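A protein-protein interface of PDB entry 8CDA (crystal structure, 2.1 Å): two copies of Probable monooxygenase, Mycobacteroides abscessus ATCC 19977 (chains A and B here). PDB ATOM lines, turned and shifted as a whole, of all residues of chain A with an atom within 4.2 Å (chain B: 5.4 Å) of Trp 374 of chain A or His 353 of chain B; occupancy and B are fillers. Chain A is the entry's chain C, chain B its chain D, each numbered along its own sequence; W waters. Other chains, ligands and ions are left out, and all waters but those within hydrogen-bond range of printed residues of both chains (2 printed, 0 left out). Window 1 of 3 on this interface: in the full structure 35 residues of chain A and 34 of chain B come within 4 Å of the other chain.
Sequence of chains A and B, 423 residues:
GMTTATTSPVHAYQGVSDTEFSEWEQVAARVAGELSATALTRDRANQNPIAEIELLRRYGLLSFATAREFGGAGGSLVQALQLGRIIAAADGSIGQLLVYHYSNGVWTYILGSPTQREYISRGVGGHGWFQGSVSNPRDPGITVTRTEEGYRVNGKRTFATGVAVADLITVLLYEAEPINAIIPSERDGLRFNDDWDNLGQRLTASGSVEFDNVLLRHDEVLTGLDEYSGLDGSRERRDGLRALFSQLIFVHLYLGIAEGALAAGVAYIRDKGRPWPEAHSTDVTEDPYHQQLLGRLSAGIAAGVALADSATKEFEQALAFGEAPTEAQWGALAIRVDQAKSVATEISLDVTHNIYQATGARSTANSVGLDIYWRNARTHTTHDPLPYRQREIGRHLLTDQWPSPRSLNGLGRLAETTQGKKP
Leu 349 of chain A touches His 353 of chain B, and with the chains exchanged His 353 of chain A touches Leu 349 of chain B.
His 353 of chain A touches its own counterpart, His 353 of chain B.
His 353 of chain A touches Trp 374 of chain B, and with the chains exchanged Trp 374 of chain A touches His 353 of chain B.
Trp 374 of chain B touches its own counterpart, Trp 374 of chain A.
Positions printed for both chains: 349, 352, 353, 371 and 374.
Printed residues of chain B within 4 Å of Leu 199 of chain A: Tyr 356 (3.7 Å) and Asp 371 (3.4 Å).
Thr 352 of chain A touches none of the printed residues of chain B.
Of the printed residues of chain B, His 353 of chain A touches Leu 349, His 353 and Trp 374.
Trp 374 of chain A touches two residues of chain B.
Of the printed residues of chain B, Arg 378 of chain A touches His 353 and Tyr 356.
Asp 350 of chain B touches none of the printed residues of chain A.
His 353 of chain B touches just these residues of chain A: Leu 349, His 353, Trp 374 and Arg 378.
Printed residues of chain A within 4 Å of Tyr 356 of chain B: Leu 199 and Arg 378.
Of the printed residues of chain A, Trp 374 of chain B touches His 353 and Trp 374.
The nearest residue of chain B that does not touch Trp 374 of chain A is Tyr 356 of chain B (4.1 Å).
The nearest printed residue of chain A that does not touch His 353 of chain B is Thr 352 of chain A (5.4 Å).
Leu 199 of chain A touches Tyr 356 of chain B (CD2 to OH, 3.7 Å).
Asp 371 of chain B touches Leu 199 of chain A.
His 353 of chain B touches Leu 349 of chain A (CE1 to O, 3.7 Å).
CE1 of His 353 of chain A touches O of Leu 349 of chain B, at 3.6 Å.
His 353 of chain B touches His 353 of chain A.
Trp 374 of chain A touches Trp 374 of chain B.
Arg 378 of chain A touches Tyr 356 of chain B.
The backbone NH (N) of Asp 371 of chain B is in hydrogen-bond range of the side-chain hydroxyl (OH) of Tyr 356 of chain B, 2.8 Å away.
The backbone carbonyl oxygen of Leu 199 of chain A lies within hydrogen-bond range of the guanidinium group of Arg 375 of chain A.
Of the 12 printed residues of chain A, 5 touch a printed residue of chain B.
Printed residues of chain A that touch a printed residue of chain B: Leu 199, Leu 349, His 353, Trp 374 and Arg 378.
Hydrophobic or aromatic side chains of chain A within 4 Å of the printed part of chain B: Leu 199, Leu 349, His 353 and Trp 374.
ND1 of His 353 of chain B sits at hydrogen-bond distance from NE1 of Trp 374 of chain A, 3.0 Å away.
The guanidinium group (NH1) of Arg 378 of chain A lies within hydrogen-bond range of the backbone carbonyl oxygen (O) of His 353 of chain B (3.0 Å).
ND1 of His 353 of chain A lies within hydrogen-bond range of NE1 of Trp 374 of chain B, at 3.0 Å.
Water W1 bridges the guanidinium group of Arg 378 of chain A (2.7 Å) and the side-chain amide oxygen of Asn 354 of chain B (2.8 Å).
Water W2 lies within hydrogen-bond range of NH2 of Arg 378 of chain A and OE1 of Gln 357 of chain B.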
ATOM      1  N   LEU A 199      31.607   6.780  -3.386  1.00  0.00           N
ATOM      2  CA  LEU A 199      30.412   5.975  -3.617  1.00  0.00           C
ATOM      3  C   LEU A 199      30.412   4.740  -2.724  1.00  0.00           C
ATOM      4  O   LEU A 199      29.520   4.557  -1.888  1.00  0.00           O
ATOM      5  CB  LEU A 199      30.342   5.576  -5.094  1.00  0.00           C
ATOM      6  CG  LEU A 199      29.237   4.592  -5.486  1.00  0.00           C
ATOM      7  CD1 LEU A 199      27.886   5.166  -5.126  1.00  0.00           C
ATOM      8  CD2 LEU A 199      29.310   4.247  -6.968  1.00  0.00           C
ATOM      9  N   LEU A 349      29.620  -7.535 -10.307  1.00  0.00           N
ATOM     10  CA  LEU A 349      28.743  -6.492 -10.826  1.00  0.00           C
ATOM     11  C   LEU A 349      27.381  -7.064 -11.202  1.00  0.00           C
ATOM     12  O   LEU A 349      26.350  -6.425 -10.973  1.00  0.00           O
ATOM     13  CB  LEU A 349      29.388  -5.813 -12.035  1.00  0.00           C
ATOM     14  CG  LEU A 349      30.688  -5.044 -11.800  1.00  0.00           C
ATOM     15  CD1 LEU A 349      31.266  -4.583 -13.129  1.00  0.00           C
ATOM     16  CD2 LEU A 349      30.462  -3.859 -10.868  1.00  0.00           C
ATOM     17  N   THR A 352      25.421  -7.828  -7.653  1.00  0.00           N
ATOM     18  CA  THR A 352      25.014  -6.681  -6.843  1.00  0.00           C
ATOM     19  C   THR A 352      24.030  -5.783  -7.578  1.00  0.00           C
ATOM     20  O   THR A 352      23.229  -5.086  -6.942  1.00  0.00           O
ATOM     21  CB  THR A 352      26.241  -5.876  -6.409  1.00  0.00           C
ATOM     22  OG1 THR A 352      26.934  -5.388  -7.565  1.00  0.00           O
ATOM     23  CG2 THR A 352      27.185  -6.733  -5.571  1.00  0.00           C
ATOM     24  N   HIS A 353      24.077  -5.784  -8.910  1.00  0.00           N
ATOM     25  CA  HIS A 353      23.173  -4.965  -9.707  1.00  0.00           C
ATOM     26  C   HIS A 353      21.816  -5.636  -9.894  1.00  0.00           C
ATOM     27  O   HIS A 353      20.774  -4.978  -9.782  1.00  0.00           O
ATOM     28  CB  HIS A 353      23.830  -4.676 -11.059  1.00  0.00           C
ATOM     29  CG  HIS A 353      22.905  -4.098 -12.083  1.00  0.00           C
ATOM     30  ND1 HIS A 353      22.303  -2.867 -11.932  1.00  0.00           N
ATOM     31  CD2 HIS A 353      22.504  -4.569 -13.286  1.00  0.00           C
ATOM     32  CE1 HIS A 353      21.560  -2.611 -12.994  1.00  0.00           C
ATOM     33  NE2 HIS A 353      21.664  -3.628 -13.830  1.00  0.00           N
ATOM     34  N   ASP A 371      21.918  -1.701  -1.551  1.00  0.00           N
ATOM     35  CA  ASP A 371      22.798  -1.093  -2.540  1.00  0.00           C
ATOM     36  C   ASP A 371      24.246  -1.004  -2.085  1.00  0.00           C
ATOM     37  O   ASP A 371      25.115  -0.731  -2.921  1.00  0.00           O
ATOM     38  CB  ASP A 371      22.313   0.316  -2.870  1.00  0.00           C
ATOM     39  CG  ASP A 371      22.339   1.234  -1.662  1.00  0.00           C
ATOM     40  OD1 ASP A 371      21.751   0.862  -0.624  1.00  0.00           O
ATOM     41  OD2 ASP A 371      22.955   2.317  -1.745  1.00  0.00           O
ATOM     42  N   ILE A 372      24.530  -1.208  -0.795  1.00  0.00           N
ATOM     43  CA  ILE A 372      25.901  -1.064  -0.309  1.00  0.00           C
ATOM     44  C   ILE A 372      26.836  -2.040  -1.007  1.00  0.00           C
ATOM     45  O   ILE A 372      28.009  -1.726  -1.249  1.00  0.00           O
ATOM     46  CB  ILE A 372      25.966  -1.182   1.228  1.00  0.00           C
ATOM     47  CG1 ILE A 372      27.376  -0.861   1.729  1.00  0.00           C
ATOM     48  CG2 ILE A 372      25.555  -2.574   1.687  1.00  0.00           C
ATOM     49  CD1 ILE A 372      27.488  -0.788   3.243  1.00  0.00           C
ATOM     50  N   TYR A 373      26.340  -3.232  -1.348  1.00  0.00           N
ATOM     51  CA  TYR A 373      27.165  -4.184  -2.080  1.00  0.00           C
ATOM     52  C   TYR A 373      27.503  -3.656  -3.467  1.00  0.00           C
ATOM     53  O   TYR A 373      28.667  -3.703  -3.887  1.00  0.00           O
ATOM     54  CB  TYR A 373      26.458  -5.535  -2.158  1.00  0.00           C
ATOM     55  CG  TYR A 373      25.979  -6.022  -0.812  1.00  0.00           C
ATOM     56  CD1 TYR A 373      26.859  -6.601   0.094  1.00  0.00           C
ATOM     57  CD2 TYR A 373      24.650  -5.884  -0.436  1.00  0.00           C
ATOM     58  CE1 TYR A 373      26.426  -7.039   1.334  1.00  0.00           C
ATOM     59  CE2 TYR A 373      24.209  -6.312   0.802  1.00  0.00           C
ATOM     60  CZ  TYR A 373      25.100  -6.889   1.681  1.00  0.00           C
ATOM     61  OH  TYR A 373      24.653  -7.314   2.911  1.00  0.00           O
ATOM     62  N   TRP A 374      26.503  -3.133  -4.182  1.00  0.00           N
ATOM     63  CA  TRP A 374      26.755  -2.541  -5.493  1.00  0.00           C
ATOM     64  C   TRP A 374      27.702  -1.357  -5.383  1.00  0.00           C
ATOM     65  O   TRP A 374      28.690  -1.270  -6.121  1.00  0.00           O
ATOM     66  CB  TRP A 374      25.441  -2.114  -6.148  1.00  0.00           C
ATOM     67  CG  TRP A 374      25.626  -1.468  -7.497  1.00  0.00           C
ATOM     68  CD1 TRP A 374      25.672  -2.097  -8.710  1.00  0.00           C
ATOM     69  CD2 TRP A 374      25.782  -0.067  -7.770  1.00  0.00           C
ATOM     70  NE1 TRP A 374      25.851  -1.178  -9.717  1.00  0.00           N
ATOM     71  CE2 TRP A 374      25.919   0.075  -9.167  1.00  0.00           C
ATOM     72  CE3 TRP A 374      25.819   1.079  -6.968  1.00  0.00           C
ATOM     73  CZ2 TRP A 374      26.091   1.317  -9.779  1.00  0.00           C
ATOM     74  CZ3 TRP A 374      25.990   2.312  -7.579  1.00  0.00           C
ATOM     75  CH2 TRP A 374      26.121   2.419  -8.972  1.00  0.00           C
ATOM     76  N   ARG A 375      27.419  -0.435  -4.458  1.00  0.00           N
ATOM     77  CA  ARG A 375      28.280   0.730  -4.284  1.00  0.00           C
ATOM     78  C   ARG A 375      29.721   0.308  -4.052  1.00  0.00           C
ATOM     79  O   ARG A 375      30.650   0.913  -4.599  1.00  0.00           O
ATOM     80  CB  ARG A 375      27.775   1.592  -3.125  1.00  0.00           C
ATOM     81  CG  ARG A 375      26.425   2.247  -3.389  1.00  0.00           C
ATOM     82  CD  ARG A 375      26.094   3.316  -2.352  1.00  0.00           C
ATOM     83  NE  ARG A 375      25.646   2.757  -1.081  1.00  0.00           N
ATOM     84  CZ  ARG A 375      26.378   2.720   0.024  1.00  0.00           C
ATOM     85  NH1 ARG A 375      27.619   3.179   0.048  1.00  0.00           N
ATOM     86  NH2 ARG A 375      25.849   2.217   1.136  1.00  0.00           N
ATOM     87  N   ASN A 376      29.921  -0.753  -3.268  1.00  0.00           N
ATOM     88  CA  ASN A 376      31.266  -1.253  -3.011  1.00  0.00           C
ATOM     89  C   ASN A 376      31.862  -1.907  -4.253  1.00  0.00           C
ATOM     90  O   ASN A 376      32.975  -1.567  -4.670  1.00  0.00           O
ATOM     91  CB  ASN A 376      31.239  -2.235  -1.839  1.00  0.00           C
ATOM     92  CG  ASN A 376      31.060  -1.541  -0.500  1.00  0.00           C
ATOM     93  OD1 ASN A 376      31.307  -0.342  -0.372  1.00  0.00           O
ATOM     94  ND2 ASN A 376      30.635  -2.296   0.508  1.00  0.00           N
ATOM     95  N   ALA A 377      31.139  -2.854  -4.855  1.00  0.00           N
ATOM     96  CA  ALA A 377      31.670  -3.559  -6.018  1.00  0.00           C
ATOM     97  C   ALA A 377      31.838  -2.622  -7.211  1.00  0.00           C
ATOM     98  O   ALA A 377      32.860  -2.671  -7.904  1.00  0.00           O
ATOM     99  CB  ALA A 377      30.773  -4.742  -6.379  1.00  0.00           C
ATOM    100  N   ARG A 378      30.848  -1.762  -7.465  1.00  0.00           N
ATOM    101  CA  ARG A 378      30.956  -0.817  -8.573  1.00  0.00           C
ATOM    102  C   ARG A 378      32.135   0.130  -8.391  1.00  0.00           C
ATOM    103  O   ARG A 378      32.770   0.529  -9.375  1.00  0.00           O
ATOM    104  CB  ARG A 378      29.653  -0.029  -8.730  1.00  0.00           C
ATOM    105  CG  ARG A 378      29.643   0.998  -9.861  1.00  0.00           C
ATOM    106  CD  ARG A 378      29.666   0.335 -11.233  1.00  0.00           C
ATOM    107  NE  ARG A 378      31.004  -0.099 -11.620  1.00  0.00           N
ATOM    108  CZ  ARG A 378      31.298  -0.682 -12.773  1.00  0.00           C
ATOM    109  NH1 ARG A 378      30.373  -0.895 -13.694  1.00  0.00           N
ATOM    110  NH2 ARG A 378      32.551  -1.065 -13.007  1.00  0.00           N
ATOM    111  N   SER B 348      18.031   1.188 -19.515  1.00  0.00           N
ATOM    112  CA  SER B 348      18.309   2.137 -18.439  1.00  0.00           C
ATOM    113  C   SER B 348      19.174   1.507 -17.354  1.00  0.00           C
ATOM    114  O   SER B 348      20.084   2.155 -16.824  1.00  0.00           O
ATOM    115  CB  SER B 348      17.007   2.685 -17.851  1.00  0.00           C
ATOM    116  OG  SER B 348      16.331   1.700 -17.089  1.00  0.00           O
ATOM    117  N   LEU B 349      18.909   0.245 -17.011  1.00  0.00           N
ATOM    118  CA  LEU B 349      19.767  -0.451 -16.058  1.00  0.00           C
ATOM    119  C   LEU B 349      21.156  -0.683 -16.642  1.00  0.00           C
ATOM    120  O   LEU B 349      22.162  -0.575 -15.931  1.00  0.00           O
ATOM    121  CB  LEU B 349      19.124  -1.775 -15.647  1.00  0.00           C
ATOM    122  CG  LEU B 349      17.806  -1.672 -14.875  1.00  0.00           C
ATOM    123  CD1 LEU B 349      17.139  -3.034 -14.777  1.00  0.00           C
ATOM    124  CD2 LEU B 349      18.038  -1.085 -13.485  1.00  0.00           C
ATOM    125  N   ASP B 350      21.224  -0.992 -17.937  1.00  0.00           N
ATOM    126  CA  ASP B 350      22.500  -1.217 -18.606  1.00  0.00           C
ATOM    127  C   ASP B 350      23.347   0.053 -18.609  1.00  0.00           C
ATOM    128  O   ASP B 350      24.526   0.027 -18.238  1.00  0.00           O
ATOM    129  CB  ASP B 350      22.223  -1.693 -20.037  1.00  0.00           C
ATOM    130  CG  ASP B 350      23.464  -2.195 -20.758  1.00  0.00           C
ATOM    131  OD1 ASP B 350      24.588  -2.069 -20.226  1.00  0.00           O
ATOM    132  OD2 ASP B 350      23.307  -2.725 -21.879  1.00  0.00           O
ATOM    133  N   VAL B 351      22.757   1.177 -19.022  1.00  0.00           N
ATOM    134  CA  VAL B 351      23.508   2.426 -19.135  1.00  0.00           C
ATOM    135  C   VAL B 351      24.017   2.873 -17.769  1.00  0.00           C
ATOM    136  O   VAL B 351      25.217   3.101 -17.576  1.00  0.00           O
ATOM    137  CB  VAL B 351      22.650   3.521 -19.793  1.00  0.00           C
ATOM    138  CG1 VAL B 351      23.348   4.871 -19.665  1.00  0.00           C
ATOM    139  CG2 VAL B 351      22.375   3.192 -21.259  1.00  0.00           C
ATOM    140  N   THR B 352      23.107   3.024 -16.806  1.00  0.00           N
ATOM    141  CA  THR B 352      23.474   3.628 -15.530  1.00  0.00           C
ATOM    142  C   THR B 352      24.443   2.770 -14.733  1.00  0.00           C
ATOM    143  O   THR B 352      25.146   3.294 -13.863  1.00  0.00           O
ATOM    144  CB  THR B 352      22.222   3.913 -14.701  1.00  0.00           C
ATOM    145  OG1 THR B 352      21.551   2.682 -14.405  1.00  0.00           O
ATOM    146  CG2 THR B 352      21.277   4.835 -15.456  1.00  0.00           C
ATOM    147  N   HIS B 353      24.500   1.473 -15.015  1.00  0.00           N
ATOM    148  CA  HIS B 353      25.371   0.552 -14.300  1.00  0.00           C
ATOM    149  C   HIS B 353      26.735   0.424 -14.968  1.00  0.00           C
ATOM    150  O   HIS B 353      27.763   0.430 -14.282  1.00  0.00           O
ATOM    151  CB  HIS B 353      24.673  -0.807 -14.188  1.00  0.00           C
ATOM    152  CG  HIS B 353      25.572  -1.939 -13.805  1.00  0.00           C
ATOM    153  ND1 HIS B 353      26.163  -2.035 -12.562  1.00  0.00           N
ATOM    154  CD2 HIS B 353      25.955  -3.041 -14.491  1.00  0.00           C
ATOM    155  CE1 HIS B 353      26.883  -3.142 -12.506  1.00  0.00           C
ATOM    156  NE2 HIS B 353      26.772  -3.771 -13.662  1.00  0.00           N
ATOM    157  N   ASN B 354      26.770   0.349 -16.297  1.00  0.00           N
ATOM    158  CA  ASN B 354      28.022   0.151 -17.014  1.00  0.00           C
ATOM    159  C   ASN B 354      28.757   1.445 -17.344  1.00  0.00           C
ATOM    160  O   ASN B 354      29.891   1.383 -17.832  1.00  0.00           O
ATOM    161  CB  ASN B 354      27.785  -0.664 -18.288  1.00  0.00           C
ATOM    162  CG  ASN B 354      27.416  -2.096 -17.989  1.00  0.00           C
ATOM    163  OD1 ASN B 354      28.233  -2.858 -17.469  1.00  0.00           O
ATOM    164  ND2 ASN B 354      26.181  -2.471 -18.303  1.00  0.00           N
ATOM    165  N   ILE B 355      28.155   2.609 -17.082  1.00  0.00           N
ATOM    166  CA  ILE B 355      28.824   3.867 -17.404  1.00  0.00           C
ATOM    167  C   ILE B 355      30.118   4.022 -16.611  1.00  0.00           C
ATOM    168  O   ILE B 355      31.066   4.670 -17.073  1.00  0.00           O
ATOM    169  CB  ILE B 355      27.862   5.062 -17.220  1.00  0.00           C
ATOM    170  CG1 ILE B 355      28.434   6.322 -17.869  1.00  0.00           C
ATOM    171  CG2 ILE B 355      27.569   5.308 -15.748  1.00  0.00           C
ATOM    172  CD1 ILE B 355      28.434   6.279 -19.384  1.00  0.00           C
ATOM    173  N   TYR B 356      30.193   3.410 -15.424  1.00  0.00           N
ATOM    174  CA  TYR B 356      31.377   3.550 -14.583  1.00  0.00           C
ATOM    175  C   TYR B 356      32.597   2.863 -15.185  1.00  0.00           C
ATOM    176  O   TYR B 356      33.731   3.253 -14.884  1.00  0.00           O
ATOM    177  CB  TYR B 356      31.103   3.002 -13.183  1.00  0.00           C
ATOM    178  CG  TYR B 356      30.480   4.003 -12.239  1.00  0.00           C
ATOM    179  CD1 TYR B 356      31.262   4.949 -11.590  1.00  0.00           C
ATOM    180  CD2 TYR B 356      29.113   3.999 -11.989  1.00  0.00           C
ATOM    181  CE1 TYR B 356      30.702   5.867 -10.721  1.00  0.00           C
ATOM    182  CE2 TYR B 356      28.542   4.913 -11.119  1.00  0.00           C
ATOM    183  CZ  TYR B 356      29.344   5.844 -10.488  1.00  0.00           C
ATOM    184  OH  TYR B 356      28.788   6.757  -9.623  1.00  0.00           O
ATOM    185  N   GLN B 357      32.395   1.841 -16.022  1.00  0.00           N
ATOM    186  CA  GLN B 357      33.535   1.169 -16.637  1.00  0.00           C
ATOM    187  C   GLN B 357      34.332   2.119 -17.523  1.00  0.00           C
ATOM    188  O   GLN B 357      35.552   1.967 -17.661  1.00  0.00           O
ATOM    189  CB  GLN B 357      33.074  -0.057 -17.428  1.00  0.00           C
ATOM    190  CG  GLN B 357      34.220  -0.871 -18.015  1.00  0.00           C
ATOM    191  CD  GLN B 357      33.746  -2.060 -18.823  1.00  0.00           C
ATOM    192  OE1 GLN B 357      33.419  -3.110 -18.268  1.00  0.00           O
ATOM    193  NE2 GLN B 357      33.709  -1.904 -20.141  1.00  0.00           N
ATOM    194  N   ASP B 371      26.386   8.120  -9.662  1.00  0.00           N
ATOM    195  CA  ASP B 371      25.525   7.021  -9.251  1.00  0.00           C
ATOM    196  C   ASP B 371      24.067   7.429  -9.099  1.00  0.00           C
ATOM    197  O   ASP B 371      23.215   6.551  -8.932  1.00  0.00           O
ATOM    198  CB  ASP B 371      26.014   6.452  -7.920  1.00  0.00           C
ATOM    199  CG  ASP B 371      25.910   7.454  -6.786  1.00  0.00           C
ATOM    200  OD1 ASP B 371      26.484   8.557  -6.904  1.00  0.00           O
ATOM    201  OD2 ASP B 371      25.238   7.142  -5.784  1.00  0.00           O
ATOM    202  N   TRP B 374      21.853   5.579 -11.598  1.00  0.00           N
ATOM    203  CA  TRP B 374      21.593   4.184 -11.256  1.00  0.00           C
ATOM    204  C   TRP B 374      20.616   4.078 -10.094  1.00  0.00           C
ATOM    205  O   TRP B 374      19.660   3.299 -10.147  1.00  0.00           O
ATOM    206  CB  TRP B 374      22.901   3.454 -10.939  1.00  0.00           C
ATOM    207  CG  TRP B 374      22.701   2.017 -10.537  1.00  0.00           C
ATOM    208  CD1 TRP B 374      22.628   0.938 -11.367  1.00  0.00           C
ATOM    209  CD2 TRP B 374      22.543   1.507  -9.203  1.00  0.00           C
ATOM    210  NE1 TRP B 374      22.437  -0.211 -10.637  1.00  0.00           N
ATOM    211  CE2 TRP B 374      22.380   0.110  -9.308  1.00  0.00           C
ATOM    212  CE3 TRP B 374      22.521   2.094  -7.935  1.00  0.00           C
ATOM    213  CZ2 TRP B 374      22.199  -0.707  -8.192  1.00  0.00           C
ATOM    214  CZ3 TRP B 374      22.342   1.280  -6.825  1.00  0.00           C
ATOM    215  CH2 TRP B 374      22.187  -0.104  -6.961  1.00  0.00           C
HETATM  216  O   HOH W   1      30.621  -2.201 -16.096  1.00  0.00           O
HETATM  217  O   HOH W   2      34.051  -2.576 -14.932  1.00  0.00           O
